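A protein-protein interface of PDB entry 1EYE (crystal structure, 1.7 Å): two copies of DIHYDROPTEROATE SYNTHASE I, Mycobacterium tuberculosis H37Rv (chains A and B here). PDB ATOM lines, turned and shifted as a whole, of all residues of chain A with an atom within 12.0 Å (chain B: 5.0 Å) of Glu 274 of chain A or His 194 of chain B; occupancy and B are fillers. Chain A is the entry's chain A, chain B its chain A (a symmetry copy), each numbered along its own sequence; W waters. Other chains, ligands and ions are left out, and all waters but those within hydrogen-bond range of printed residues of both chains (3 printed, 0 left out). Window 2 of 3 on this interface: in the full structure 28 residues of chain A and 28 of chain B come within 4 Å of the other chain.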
ATOM      1  N   LEU A 246      30.419   6.386  17.703  1.00  0.00           N
ATOM      2  CA  LEU A 246      30.314   5.284  16.765  1.00  0.00           C
ATOM      3  C   LEU A 246      31.627   4.514  16.585  1.00  0.00           C
ATOM      4  O   LEU A 246      31.655   3.342  16.225  1.00  0.00           O
ATOM      5  CB  LEU A 246      29.985   5.850  15.372  1.00  0.00           C
ATOM      6  CG  LEU A 246      28.520   6.151  15.185  1.00  0.00           C
ATOM      7  CD1 LEU A 246      28.334   6.696  13.762  1.00  0.00           C
ATOM      8  CD2 LEU A 246      27.717   4.860  15.404  1.00  0.00           C
ATOM      9  N   ILE A 264      24.797  12.256  21.315  1.00  0.00           N
ATOM     10  CA  ILE A 264      24.994  10.947  21.907  1.00  0.00           C
ATOM     11  C   ILE A 264      23.674  10.212  22.097  1.00  0.00           C
ATOM     12  O   ILE A 264      23.533   9.018  21.804  1.00  0.00           O
ATOM     13  CB  ILE A 264      25.845  11.019  23.178  1.00  0.00           C
ATOM     14  CG1 ILE A 264      27.212  11.598  22.793  1.00  0.00           C
ATOM     15  CG2 ILE A 264      25.994   9.591  23.720  1.00  0.00           C
ATOM     16  CD1 ILE A 264      28.138  11.942  23.972  1.00  0.00           C
ATOM     17  N   LYS A 265      22.687  10.943  22.567  1.00  0.00           N
ATOM     18  CA  LYS A 265      21.367  10.335  22.728  1.00  0.00           C
ATOM     19  C   LYS A 265      20.845   9.822  21.370  1.00  0.00           C
ATOM     20  O   LYS A 265      20.279   8.721  21.258  1.00  0.00           O
ATOM     21  CB  LYS A 265      20.383  11.342  23.320  1.00  0.00           C
ATOM     22  CG  LYS A 265      20.734  11.754  24.742  1.00  0.00           C
ATOM     23  CD  LYS A 265      19.748  12.719  25.376  1.00  0.00           C
ATOM     24  CE  LYS A 265      20.016  12.920  26.869  1.00  0.00           C
ATOM     25  NZ  LYS A 265      19.398  14.148  27.402  1.00  0.00           N
ATOM     26  N   VAL A 266      21.073  10.623  20.313  1.00  0.00           N
ATOM     27  CA  VAL A 266      20.630  10.222  18.976  1.00  0.00           C
ATOM     28  C   VAL A 266      21.310   8.918  18.543  1.00  0.00           C
ATOM     29  O   VAL A 266      20.691   7.957  18.070  1.00  0.00           O
ATOM     30  CB  VAL A 266      20.857  11.307  17.889  1.00  0.00           C
ATOM     31  CG1 VAL A 266      20.576  10.751  16.478  1.00  0.00           C
ATOM     32  CG2 VAL A 266      19.940  12.525  18.103  1.00  0.00           C
ATOM     33  N   VAL A 267      22.633   8.899  18.674  1.00  0.00           N
ATOM     34  CA  VAL A 267      23.387   7.738  18.267  1.00  0.00           C
ATOM     35  C   VAL A 267      22.883   6.512  18.995  1.00  0.00           C
ATOM     36  O   VAL A 267      22.676   5.454  18.407  1.00  0.00           O
ATOM     37  CB  VAL A 267      24.875   7.904  18.528  1.00  0.00           C
ATOM     38  CG1 VAL A 267      25.530   6.568  18.228  1.00  0.00           C
ATOM     39  CG2 VAL A 267      25.418   8.961  17.587  1.00  0.00           C
ATOM     40  N   GLU A 268      22.681   6.655  20.293  1.00  0.00           N
ATOM     41  CA  GLU A 268      22.228   5.525  21.066  1.00  0.00           C
ATOM     42  C   GLU A 268      20.826   5.098  20.683  1.00  0.00           C
ATOM     43  O   GLU A 268      20.528   3.905  20.645  1.00  0.00           O
ATOM     44  CB  GLU A 268      22.247   5.821  22.569  1.00  0.00           C
ATOM     45  CG  GLU A 268      21.211   4.975  23.340  1.00  0.00           C
ATOM     46  CD  GLU A 268      21.417   5.027  24.834  1.00  0.00           C
ATOM     47  OE1 GLU A 268      20.833   4.277  25.611  1.00  0.00           O
ATOM     48  OE2 GLU A 268      22.283   5.954  25.207  1.00  0.00           O
ATOM     49  N   ALA A 269      19.962   6.071  20.419  1.00  0.00           N
ATOM     50  CA  ALA A 269      18.625   5.708  20.014  1.00  0.00           C
ATOM     51  C   ALA A 269      18.664   5.028  18.651  1.00  0.00           C
ATOM     52  O   ALA A 269      18.005   4.020  18.413  1.00  0.00           O
ATOM     53  CB  ALA A 269      17.727   6.927  20.016  1.00  0.00           C
ATOM     54  N   TRP A 270      19.455   5.553  17.737  1.00  0.00           N
ATOM     55  CA  TRP A 270      19.525   4.961  16.423  1.00  0.00           C
ATOM     56  C   TRP A 270      20.166   3.586  16.458  1.00  0.00           C
ATOM     57  O   TRP A 270      19.623   2.587  15.985  1.00  0.00           O
ATOM     58  CB  TRP A 270      20.299   5.895  15.487  1.00  0.00           C
ATOM     59  CG  TRP A 270      20.484   5.482  14.051  1.00  0.00           C
ATOM     60  CD1 TRP A 270      20.998   4.321  13.579  1.00  0.00           C
ATOM     61  CD2 TRP A 270      20.238   6.301  12.892  1.00  0.00           C
ATOM     62  NE1 TRP A 270      21.039   4.346  12.197  1.00  0.00           N
ATOM     63  CE2 TRP A 270      20.595   5.559  11.752  1.00  0.00           C
ATOM     64  CE3 TRP A 270      19.753   7.593  12.711  1.00  0.00           C
ATOM     65  CZ2 TRP A 270      20.479   6.078  10.456  1.00  0.00           C
ATOM     66  CZ3 TRP A 270      19.644   8.099  11.435  1.00  0.00           C
ATOM     67  CH2 TRP A 270      19.989   7.347  10.314  1.00  0.00           C
ATOM     68  N   MET A 271      21.358   3.523  17.015  1.00  0.00           N
ATOM     69  CA  MET A 271      22.084   2.264  17.070  1.00  0.00           C
ATOM     70  C   MET A 271      21.452   1.172  17.912  1.00  0.00           C
ATOM     71  O   MET A 271      21.731  -0.014  17.702  1.00  0.00           O
ATOM     72  CB  MET A 271      23.568   2.485  17.409  1.00  0.00           C
ATOM     73  CG  MET A 271      24.224   3.358  16.339  1.00  0.00           C
ATOM     74  SD  MET A 271      24.237   2.550  14.714  1.00  0.00           S
ATOM     75  CE  MET A 271      25.358   1.162  15.067  1.00  0.00           C
ATOM     76  N   GLY A 272      20.607   1.555  18.862  1.00  0.00           N
ATOM     77  CA  GLY A 272      19.991   0.534  19.672  1.00  0.00           C
ATOM     78  C   GLY A 272      18.604   0.115  19.164  1.00  0.00           C
ATOM     79  O   GLY A 272      17.934  -0.692  19.804  1.00  0.00           O
ATOM     80  N   ALA A 273      18.138   0.659  18.032  1.00  0.00           N
ATOM     81  CA  ALA A 273      16.788   0.333  17.571  1.00  0.00           C
ATOM     82  C   ALA A 273      16.516  -1.022  16.965  1.00  0.00           C
ATOM     83  O   ALA A 273      16.059  -1.132  15.831  1.00  0.00           O
ATOM     84  CB  ALA A 273      16.005   1.449  16.917  1.00  0.00           C
ATOM     85  N   GLU A 274      16.781  -2.037  17.783  1.00  0.00           N
ATOM     86  CA  GLU A 274      16.560  -3.446  17.500  1.00  0.00           C
ATOM     87  C   GLU A 274      16.449  -3.711  16.015  1.00  0.00           C
ATOM     88  O   GLU A 274      15.770  -4.660  15.637  1.00  0.00           O
ATOM     89  CB  GLU A 274      15.298  -3.976  18.216  1.00  0.00           C
ATOM     90  CG  GLU A 274      15.045  -3.334  19.598  1.00  0.00           C
ATOM     91  CD  GLU A 274      14.617  -1.888  19.537  1.00  0.00           C
ATOM     92  OE1 GLU A 274      14.072  -1.392  18.556  1.00  0.00           O
ATOM     93  OE2 GLU A 274      15.005  -1.195  20.590  1.00  0.00           O
ATOM     94  N   GLN B 187       9.331   4.931  18.861  1.00  0.00           N
ATOM     95  CA  GLN B 187       9.974   3.632  18.712  1.00  0.00           C
ATOM     96  C   GLN B 187       9.991   3.165  17.262  1.00  0.00           C
ATOM     97  O   GLN B 187      11.020   2.677  16.783  1.00  0.00           O
ATOM     98  CB  GLN B 187       9.452   2.548  19.658  1.00  0.00           C
ATOM     99  CG  GLN B 187      10.204   2.563  21.017  1.00  0.00           C
ATOM    100  CD  GLN B 187      11.683   2.990  20.970  1.00  0.00           C
ATOM    101  OE1 GLN B 187      12.539   2.287  20.398  1.00  0.00           O
ATOM    102  NE2 GLN B 187      12.024   4.111  21.632  1.00  0.00           N
ATOM    103  N   TRP B 190      12.684   5.175  15.395  1.00  0.00           N
ATOM    104  CA  TRP B 190      14.050   4.712  15.620  1.00  0.00           C
ATOM    105  C   TRP B 190      14.320   3.410  14.894  1.00  0.00           C
ATOM    106  O   TRP B 190      15.418   3.200  14.346  1.00  0.00           O
ATOM    107  CB  TRP B 190      14.427   4.658  17.112  1.00  0.00           C
ATOM    108  CG  TRP B 190      14.430   6.024  17.728  1.00  0.00           C
ATOM    109  CD1 TRP B 190      13.613   6.437  18.709  1.00  0.00           C
ATOM    110  CD2 TRP B 190      15.302   7.130  17.429  1.00  0.00           C
ATOM    111  NE1 TRP B 190      13.888   7.734  19.038  1.00  0.00           N
ATOM    112  CE2 TRP B 190      14.910   8.195  18.266  1.00  0.00           C
ATOM    113  CE3 TRP B 190      16.357   7.313  16.525  1.00  0.00           C
ATOM    114  CZ2 TRP B 190      15.542   9.433  18.251  1.00  0.00           C
ATOM    115  CZ3 TRP B 190      16.972   8.546  16.491  1.00  0.00           C
ATOM    116  CH2 TRP B 190      16.579   9.587  17.358  1.00  0.00           C
ATOM    117  N   ALA B 191      13.295   2.554  14.843  1.00  0.00           N
ATOM    118  CA  ALA B 191      13.423   1.274  14.161  1.00  0.00           C
ATOM    119  C   ALA B 191      13.665   1.459  12.669  1.00  0.00           C
ATOM    120  O   ALA B 191      14.507   0.800  12.033  1.00  0.00           O
ATOM    121  CB  ALA B 191      12.180   0.430  14.383  1.00  0.00           C
ATOM    122  N   ILE B 192      12.926   2.405  12.112  1.00  0.00           N
ATOM    123  CA  ILE B 192      13.063   2.709  10.690  1.00  0.00           C
ATOM    124  C   ILE B 192      14.438   3.258  10.402  1.00  0.00           C
ATOM    125  O   ILE B 192      15.075   2.845   9.440  1.00  0.00           O
ATOM    126  CB  ILE B 192      11.966   3.649  10.184  1.00  0.00           C
ATOM    127  CG1 ILE B 192      10.621   2.913  10.162  1.00  0.00           C
ATOM    128  CG2 ILE B 192      12.344   4.189   8.794  1.00  0.00           C
ATOM    129  CD1 ILE B 192       9.426   3.858  10.307  1.00  0.00           C
ATOM    130  N   LEU B 193      14.903   4.180  11.242  1.00  0.00           N
ATOM    131  CA  LEU B 193      16.242   4.735  11.026  1.00  0.00           C
ATOM    132  C   LEU B 193      17.340   3.702  11.173  1.00  0.00           C
ATOM    133  O   LEU B 193      18.261   3.599  10.364  1.00  0.00           O
ATOM    134  CB  LEU B 193      16.519   5.944  11.926  1.00  0.00           C
ATOM    135  CG  LEU B 193      15.571   7.086  11.566  1.00  0.00           C
ATOM    136  CD1 LEU B 193      15.659   8.157  12.656  1.00  0.00           C
ATOM    137  CD2 LEU B 193      15.939   7.672  10.179  1.00  0.00           C
ATOM    138  N   HIS B 194      17.228   2.895  12.206  1.00  0.00           N
ATOM    139  CA  HIS B 194      18.221   1.856  12.378  1.00  0.00           C
ATOM    140  C   HIS B 194      18.317   0.976  11.126  1.00  0.00           C
ATOM    141  O   HIS B 194      19.382   0.598  10.685  1.00  0.00           O
ATOM    142  CB  HIS B 194      17.792   1.046  13.607  1.00  0.00           C
ATOM    143  CG  HIS B 194      18.781   0.025  14.018  1.00  0.00           C
ATOM    144  ND1 HIS B 194      18.612  -1.295  13.676  1.00  0.00           N
ATOM    145  CD2 HIS B 194      19.918   0.133  14.727  1.00  0.00           C
ATOM    146  CE1 HIS B 194      19.631  -1.960  14.194  1.00  0.00           C
ATOM    147  NE2 HIS B 194      20.432  -1.125  14.832  1.00  0.00           N
ATOM    148  N   ALA B 195      17.186   0.639  10.509  1.00  0.00           N
ATOM    149  CA  ALA B 195      17.157  -0.194   9.320  1.00  0.00           C
ATOM    150  C   ALA B 195      17.190   0.651   8.054  1.00  0.00           C
ATOM    151  O   ALA B 195      16.717   0.273   6.978  1.00  0.00           O
ATOM    152  CB  ALA B 195      15.864  -0.987   9.341  1.00  0.00           C
ATOM    153  N   LEU B 196      17.725   1.849   8.162  1.00  0.00           N
ATOM    154  CA  LEU B 196      17.750   2.661   6.976  1.00  0.00           C
ATOM    155  C   LEU B 196      18.393   1.980   5.783  1.00  0.00           C
ATOM    156  O   LEU B 196      17.946   2.108   4.649  1.00  0.00           O
ATOM    157  CB  LEU B 196      18.411   4.009   7.267  1.00  0.00           C
ATOM    158  CG  LEU B 196      18.370   4.976   6.105  1.00  0.00           C
ATOM    159  CD1 LEU B 196      16.927   5.299   5.747  1.00  0.00           C
ATOM    160  CD2 LEU B 196      19.098   6.253   6.515  1.00  0.00           C
ATOM    161  N   PRO B 197      19.473   1.257   6.019  1.00  0.00           N
ATOM    162  CA  PRO B 197      20.149   0.601   4.907  1.00  0.00           C
ATOM    163  C   PRO B 197      19.265  -0.377   4.145  1.00  0.00           C
ATOM    164  O   PRO B 197      19.378  -0.518   2.936  1.00  0.00           O
ATOM    165  CB  PRO B 197      21.427  -0.025   5.478  1.00  0.00           C
ATOM    166  CG  PRO B 197      21.667   0.691   6.801  1.00  0.00           C
ATOM    167  CD  PRO B 197      20.312   1.217   7.258  1.00  0.00           C
HETATM  168  O   HOH W   1      15.212  -1.627  13.012  1.00  0.00           O
HETATM  169  O   HOH W   2      21.523   2.138  10.585  1.00  0.00           O
HETATM  170  O   HOH W   3      12.957   1.538  18.115  1.00  0.00           O
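The indole nitrogen (NE1) of Trp 270 of chain A sits close to the backbone carbonyl oxygen (O) of Leu 193 of chain B, 3.4 Å away. O of Met 271 of chain A sits at hydrogen-bond distance from NE2 of His 194 of chain B (3.3 Å). ND1 of His 194 of chain B sits at hydrogen-bond distance from O of Ala 273 of chain A, 3.3 Å away.
Among the printed residues, merely in contact across the chains: Ala 269 of chain A with Trp 190 of chain B, Trp 270 of chain A with Trp 190 of chain B, Trp 270 of chain A with His 194 of chain B, Ala 273 of chain A with Trp 190 of chain B, Ala 273 of chain A with Ala 191 of chain B and Glu 274 of chain A with His 194 of chain B.
Of the printed residues of chain B, Glu 274 of chain A touches His 194 (3.998 Å). Printed residues of chain A within 4 Å of His 194 of chain B: Trp 270 (2.8 Å), Met 271 (3.3 Å), Ala 273 (3.3 Å) and Glu 274 (3.998 Å). No residue of chain A comes within 4 Å of Gln 187 of chain B. Ala 191 of chain B touches one residue of chain A. Pro 197 of chain B touches none of the printed residues of chain A. Of the printed residues of chain B, Met 271 of chain A touches His 194. Of the printed residues of chain B, Ala 269 of chain A touches Trp 190 (3.6 Å). Of the printed residues of chain A, Trp 190 of chain B touches Ala 269, Trp 270 and Ala 273. Of the printed residues of chain B, Trp 270 of chain A touches Trp 190, Leu 193 and His 194. Of the printed residues of chain B, Ala 273 of chain A touches Trp 190, Ala 191 and His 194. Leu 246 of chain A touches none of the printed residues of chain B. The nearest printed residue of chain A that does not touch His 194 of chain B is Gly 272 of chain A (4.4 Å).
Of the 12 printed residues of chain A, 5 touch a printed residue of chain B.
No position is printed for both chains. Of the 9 pairs that touch across the chains among the printed residues, none has its exchanged pair printed and touching as well.
Water W3 lies within hydrogen-bond range of the side-chain amide oxygen of Gln 187 of chain B (2.4 Å), the side-chain carboxylate of Glu 274 of chain A (3.2 Å) and the backbone NH of Ala 191 of chain B (3.4 Å). Water W2 bridges the backbone carbonyl oxygen of His 194 of chain B and the indole nitrogen of Trp 270 of chain A. Water W1 lies within hydrogen-bond range of O of Ala 191 of chain B, O of Ala 273 of chain A and ND1 of His 194 of chain B.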
